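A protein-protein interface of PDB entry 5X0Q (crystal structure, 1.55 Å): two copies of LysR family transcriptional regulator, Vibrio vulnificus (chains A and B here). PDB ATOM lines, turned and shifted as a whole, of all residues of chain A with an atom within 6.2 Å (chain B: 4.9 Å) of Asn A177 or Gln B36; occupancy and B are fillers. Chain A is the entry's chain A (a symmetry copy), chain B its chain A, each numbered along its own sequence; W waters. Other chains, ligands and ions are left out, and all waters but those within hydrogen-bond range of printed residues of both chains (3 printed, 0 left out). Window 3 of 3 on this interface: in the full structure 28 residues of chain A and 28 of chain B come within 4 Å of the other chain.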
ATOM      1  N   ALA A 157      -8.496  -4.698 -14.387  1.00  0.00           N
ATOM      2  CA  ALA A 157      -9.929  -4.631 -14.634  1.00  0.00           C
ATOM      3  C   ALA A 157     -10.552  -3.392 -14.020  1.00  0.00           C
ATOM      4  O   ALA A 157     -11.574  -2.897 -14.519  1.00  0.00           O
ATOM      5  CB  ALA A 157     -10.600  -5.932 -14.126  1.00  0.00           C
ATOM      6  N   ASN A 158      -9.954  -2.861 -12.938  1.00  0.00           N
ATOM      7  CA  ASN A 158     -10.387  -1.631 -12.302  1.00  0.00           C
ATOM      8  C   ASN A 158      -9.957  -0.396 -13.085  1.00  0.00           C
ATOM      9  O   ASN A 158     -10.361   0.714 -12.743  1.00  0.00           O
ATOM     10  CB  ASN A 158      -9.809  -1.636 -10.858  1.00  0.00           C
ATOM     11  CG  ASN A 158     -10.295  -0.499  -9.981  1.00  0.00           C
ATOM     12  OD1 ASN A 158      -9.469   0.113  -9.283  1.00  0.00           O
ATOM     13  ND2 ASN A 158     -11.597  -0.228  -9.946  1.00  0.00           N
ATOM     14  N   GLY A 173      -9.854 -19.145 -18.434  1.00  0.00           N
ATOM     15  CA  GLY A 173     -10.949 -18.289 -18.020  1.00  0.00           C
ATOM     16  C   GLY A 173     -10.608 -17.197 -17.025  1.00  0.00           C
ATOM     17  O   GLY A 173     -11.539 -16.609 -16.445  1.00  0.00           O
ATOM     18  N   LEU A 175      -9.820 -14.213 -17.348  1.00  0.00           N
ATOM     19  CA  LEU A 175     -10.367 -12.890 -17.651  1.00  0.00           C
ATOM     20  C   LEU A 175     -11.892 -12.897 -17.686  1.00  0.00           C
ATOM     21  O   LEU A 175     -12.483 -11.826 -17.887  1.00  0.00           O
ATOM     22  CB  LEU A 175      -9.849 -12.375 -19.005  1.00  0.00           C
ATOM     23  CG  LEU A 175      -8.347 -12.578 -19.203  1.00  0.00           C
ATOM     24  CD1 LEU A 175      -7.951 -12.021 -20.552  1.00  0.00           C
ATOM     25  CD2 LEU A 175      -7.501 -11.965 -18.097  1.00  0.00           C
ATOM     26  N   ASP A 176     -12.549 -14.039 -17.460  1.00  0.00           N
ATOM     27  CA  ASP A 176     -14.011 -14.080 -17.615  1.00  0.00           C
ATOM     28  C   ASP A 176     -14.719 -13.047 -16.727  1.00  0.00           C
ATOM     29  O   ASP A 176     -14.413 -12.905 -15.532  1.00  0.00           O
ATOM     30  CB  ASP A 176     -14.551 -15.462 -17.250  1.00  0.00           C
ATOM     31  CG  ASP A 176     -14.362 -16.484 -18.365  1.00  0.00           C
ATOM     32  OD1 ASP A 176     -14.054 -16.113 -19.512  1.00  0.00           O
ATOM     33  OD2 ASP A 176     -14.552 -17.710 -18.082  1.00  0.00           O
ATOM     34  N   ASN A 177     -15.712 -12.386 -17.309  1.00  0.00           N
ATOM     35  CA  ASN A 177     -16.574 -11.440 -16.618  1.00  0.00           C
ATOM     36  C   ASN A 177     -15.828 -10.257 -16.017  1.00  0.00           C
ATOM     37  O   ASN A 177     -16.378  -9.552 -15.161  1.00  0.00           O
ATOM     38  CB  ASN A 177     -17.375 -12.155 -15.536  1.00  0.00           C
ATOM     39  CG  ASN A 177     -18.335 -13.179 -16.111  1.00  0.00           C
ATOM     40  OD1 ASN A 177     -18.448 -14.317 -15.605  1.00  0.00           O
ATOM     41  ND2 ASN A 177     -19.028 -12.804 -17.145  1.00  0.00           N
ATOM     42  N   GLN A 178     -14.602  -9.971 -16.469  1.00  0.00           N
ATOM     43  CA  GLN A 178     -13.868  -8.806 -15.986  1.00  0.00           C
ATOM     44  C   GLN A 178     -13.759  -7.706 -17.032  1.00  0.00           C
ATOM     45  O   GLN A 178     -13.106  -6.674 -16.778  1.00  0.00           O
ATOM     46  CB  GLN A 178     -12.488  -9.220 -15.477  1.00  0.00           C
ATOM     47  CG  GLN A 178     -12.627 -10.275 -14.355  1.00  0.00           C
ATOM     48  CD  GLN A 178     -11.399 -10.354 -13.472  1.00  0.00           C
ATOM     49  OE1 GLN A 178     -10.600 -11.315 -13.545  1.00  0.00           O
ATOM     50  NE2 GLN A 178     -11.222  -9.347 -12.655  1.00  0.00           N
ATOM     51  N   ASN A 179     -14.434  -7.871 -18.170  1.00  0.00           N
ATOM     52  CA  ASN A 179     -14.508  -6.837 -19.221  1.00  0.00           C
ATOM     53  C   ASN A 179     -13.128  -6.333 -19.643  1.00  0.00           C
ATOM     54  O   ASN A 179     -12.852  -5.131 -19.649  1.00  0.00           O
ATOM     55  CB  ASN A 179     -15.403  -5.667 -18.770  1.00  0.00           C
ATOM     56  CG  ASN A 179     -16.114  -5.023 -19.921  1.00  0.00           C
ATOM     57  OD1 ASN A 179     -16.195  -5.600 -21.012  1.00  0.00           O
ATOM     58  ND2 ASN A 179     -16.614  -3.805 -19.706  1.00  0.00           N
ATOM     59  N   LEU A 180     -12.252  -7.267 -20.015  1.00  0.00           N
ATOM     60  CA  LEU A 180     -10.904  -6.951 -20.462  1.00  0.00           C
ATOM     61  C   LEU A 180     -10.777  -7.195 -21.960  1.00  0.00           C
ATOM     62  O   LEU A 180     -11.579  -7.908 -22.577  1.00  0.00           O
ATOM     63  CB  LEU A 180      -9.854  -7.819 -19.759  1.00  0.00           C
ATOM     64  CG  LEU A 180      -9.975  -7.711 -18.230  1.00  0.00           C
ATOM     65  CD1 LEU A 180      -9.175  -8.781 -17.516  1.00  0.00           C
ATOM     66  CD2 LEU A 180      -9.441  -6.330 -17.927  1.00  0.00           C
ATOM     67  N   CYS B  32     -13.226 -10.000  -8.024  1.00  0.00           N
ATOM     68  CA  CYS B  32     -13.654  -9.786  -9.400  1.00  0.00           C
ATOM     69  C   CYS B  32     -14.982  -9.050  -9.434  1.00  0.00           C
ATOM     70  O   CYS B  32     -15.162  -8.089 -10.210  1.00  0.00           O
ATOM     71  CB  CYS B  32     -13.799 -11.124 -10.142  1.00  0.00           C
ATOM     72  SG  CYS B  32     -12.301 -12.099 -10.322  1.00  0.00           S
ATOM     73  N   ASP B  33     -15.945  -9.536  -8.618  1.00  0.00           N
ATOM     74  CA  ASP B  33     -17.267  -8.919  -8.537  1.00  0.00           C
ATOM     75  C   ASP B  33     -17.173  -7.520  -7.967  1.00  0.00           C
ATOM     76  O   ASP B  33     -17.833  -6.607  -8.475  1.00  0.00           O
ATOM     77  CB  ASP B  33     -18.211  -9.744  -7.651  1.00  0.00           C
ATOM     78  CG  ASP B  33     -18.293 -11.214  -8.066  1.00  0.00           C
ATOM     79  OD1 ASP B  33     -18.272 -11.479  -9.283  1.00  0.00           O
ATOM     80  OD2 ASP B  33     -18.417 -12.081  -7.160  1.00  0.00           O
ATOM     81  N   LEU B  34     -16.339  -7.345  -6.928  1.00  0.00           N
ATOM     82  CA  LEU B  34     -16.214  -6.045  -6.287  1.00  0.00           C
ATOM     83  C   LEU B  34     -15.704  -5.010  -7.277  1.00  0.00           C
ATOM     84  O   LEU B  34     -16.256  -3.916  -7.376  1.00  0.00           O
ATOM     85  CB  LEU B  34     -15.283  -6.140  -5.077  1.00  0.00           C
ATOM     86  CG  LEU B  34     -15.030  -4.789  -4.370  1.00  0.00           C
ATOM     87  CD1 LEU B  34     -16.293  -4.142  -3.818  1.00  0.00           C
ATOM     88  CD2 LEU B  34     -14.007  -5.009  -3.239  1.00  0.00           C
ATOM     89  N   VAL B  35     -14.676  -5.354  -8.055  1.00  0.00           N
ATOM     90  CA  VAL B  35     -14.135  -4.405  -9.028  1.00  0.00           C
ATOM     91  C   VAL B  35     -15.190  -4.014 -10.064  1.00  0.00           C
ATOM     92  O   VAL B  35     -15.311  -2.841 -10.428  1.00  0.00           O
ATOM     93  CB  VAL B  35     -12.874  -4.995  -9.691  1.00  0.00           C
ATOM     94  CG1 VAL B  35     -12.575  -4.250 -11.010  1.00  0.00           C
ATOM     95  CG2 VAL B  35     -11.698  -4.913  -8.716  1.00  0.00           C
ATOM     96  N   GLN B  36     -15.966  -4.972 -10.578  1.00  0.00           N
ATOM     97  CA  GLN B  36     -16.969  -4.599 -11.582  1.00  0.00           C
ATOM     98  C   GLN B  36     -18.019  -3.685 -10.975  1.00  0.00           C
ATOM     99  O   GLN B  36     -18.474  -2.740 -11.618  1.00  0.00           O
ATOM    100  CB  GLN B  36     -17.644  -5.834 -12.155  1.00  0.00           C
ATOM    101  CG  GLN B  36     -16.696  -6.726 -12.964  1.00  0.00           C
ATOM    102  CD  GLN B  36     -16.033  -5.972 -14.098  1.00  0.00           C
ATOM    103  OE1 GLN B  36     -16.710  -5.408 -14.970  1.00  0.00           O
ATOM    104  NE2 GLN B  36     -14.688  -5.955 -14.091  1.00  0.00           N
ATOM    105  N   GLU B  37     -18.378  -3.930  -9.718  1.00  0.00           N
ATOM    106  CA  GLU B  37     -19.386  -3.076  -9.108  1.00  0.00           C
ATOM    107  C   GLU B  37     -18.848  -1.672  -8.868  1.00  0.00           C
ATOM    108  O   GLU B  37     -19.548  -0.693  -9.175  1.00  0.00           O
ATOM    109  CB  GLU B  37     -19.875  -3.695  -7.802  1.00  0.00           C
ATOM    110  CG  GLU B  37     -21.023  -2.989  -7.158  1.00  0.00           C
ATOM    111  CD  GLU B  37     -22.370  -3.230  -7.843  1.00  0.00           C
ATOM    112  OE1 GLU B  37     -23.373  -2.775  -7.253  1.00  0.00           O
ATOM    113  OE2 GLU B  37     -22.442  -3.865  -8.928  1.00  0.00           O
ATOM    114  N   ILE B  38     -17.623  -1.533  -8.327  1.00  0.00           N
ATOM    115  CA  ILE B  38     -17.138  -0.183  -8.036  1.00  0.00           C
ATOM    116  C   ILE B  38     -16.784   0.564  -9.312  1.00  0.00           C
ATOM    117  O   ILE B  38     -16.866   1.804  -9.345  1.00  0.00           O
ATOM    118  CB  ILE B  38     -15.966  -0.177  -7.050  1.00  0.00           C
ATOM    119  CG1 ILE B  38     -14.716  -0.796  -7.649  1.00  0.00           C
ATOM    120  CG2 ILE B  38     -16.367  -0.824  -5.704  1.00  0.00           C
ATOM    121  CD1 ILE B  38     -13.511  -0.521  -6.754  1.00  0.00           C
ATOM    122  N   ASN B  39     -16.412  -0.145 -10.390  1.00  0.00           N
ATOM    123  CA  ASN B  39     -16.149   0.542 -11.653  1.00  0.00           C
ATOM    124  C   ASN B  39     -17.337   1.398 -12.073  1.00  0.00           C
ATOM    125  O   ASN B  39     -17.162   2.480 -12.639  1.00  0.00           O
ATOM    126  CB  ASN B  39     -15.867  -0.458 -12.778  1.00  0.00           C
ATOM    127  CG  ASN B  39     -14.441  -0.965 -12.779  1.00  0.00           C
ATOM    128  OD1 ASN B  39     -13.582  -0.446 -12.070  1.00  0.00           O
ATOM    129  ND2 ASN B  39     -14.180  -1.977 -13.606  1.00  0.00           N
ATOM    130  N   GLN B  40     -18.552   0.897 -11.848  1.00  0.00           N
ATOM    131  CA  GLN B  40     -19.754   1.613 -12.253  1.00  0.00           C
ATOM    132  C   GLN B  40     -20.242   2.533 -11.152  1.00  0.00           C
ATOM    133  O   GLN B  40     -20.527   3.708 -11.400  1.00  0.00           O
ATOM    134  CB  GLN B  40     -20.845   0.623 -12.637  1.00  0.00           C
ATOM    135  CG  GLN B  40     -22.159   1.302 -12.975  1.00  0.00           C
ATOM    136  CD  GLN B  40     -23.256   0.313 -13.264  1.00  0.00           C
ATOM    137  OE1 GLN B  40     -23.646  -0.485 -12.400  1.00  0.00           O
ATOM    138  NE2 GLN B  40     -23.767   0.350 -14.492  1.00  0.00           N
HETATM  139  O   HOH W   1     -13.236  -7.562 -12.268  1.00  0.00           O
HETATM  140  O   HOH W   2     -16.362 -10.422 -12.395  1.00  0.00           O
HETATM  141  O   HOH W   3     -13.692   2.177  -9.397  1.00  0.00           O
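Water W1 lies within hydrogen-bond range of NE2 of Gln A178 (2.7 Å), NE2 of Gln B36 (2.8 Å) and O of Cys B32 (2.9 Å). Water W2 bridges the backbone carbonyl oxygen of Asn A177 (2.9 Å) and the backbone carbonyl oxygen of Cys B32 (3.4 Å). Water W3 lies within hydrogen-bond range of O of Ile B38 and ND2 of Asn A158.
Of chain B, only Gln B36 comes within 4 Å of Asn A177. Of chain A, only Asn A177 and Gln A178 come within 4 Å of Gln B36. Of the printed residues of chain A, Asn B39 touches Ala A157 and Asn A158. Of the printed residues of chain A, Ile B38 touches Asn A158. Printed residues of chain A within 4 Å of Cys B32: Gln A178 (3.7 Å). Of the printed residues of chain B, Asn A158 touches Val B35, Ile B38 and Asn B39. Of the printed residues of chain B, Gln A178 touches Cys B32 (3.7 Å) and Gln B36 (3.2 Å). The nearest printed residue of chain B that does not touch Asn A177 is Cys B32 (5.3 Å). The nearest printed residue of chain B that does not touch Gln A178 is Val B35 (5.5 Å).
OD1 of Asn B39 is in hydrogen-bond range of ND2 of Asn A158 (2.9 Å). The backbone carbonyl oxygen of Ala A157 sits at hydrogen-bond distance from the side-chain amide nitrogen of Asn B39 (2.9 Å). SG of Cys B32 lies close to OE1 of Gln A178 (3.7 Å). The backbone carbonyl oxygen (O) of Gln A178 sits at hydrogen-bond distance from the side-chain amide nitrogen (NE2) of Gln B36 (3.2 Å).
No position is printed for both chains.
Hydrophobic or aromatic side chains of chain B within 4 Å of the printed part of chain A: Val B35 and Ile B38. Along chain A the printed residues that touch a printed residue of chain B span positions 157 to 178. Among the printed residues, 8 pairs touch across the chains. Among the printed residues, no Asp or Glu carboxylate lies within 4 Å of a Lys or Arg side-chain nitrogen of the other chain.
C of Ala A157 touches CG1 of Val B35, 3.7 Å away. Val B35 touches Asn A158 (CG1 to N, 3.5 Å). ND2 of Asn A158 touches CD1 of Ile B38, at 3.7 Å. Asn A177 touches Gln B36 (O to CG, 3.6 Å).
The side-chain amide oxygen (OD1) of Asn B39 sits close to the backbone carbonyl oxygen (O) of Val B35.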
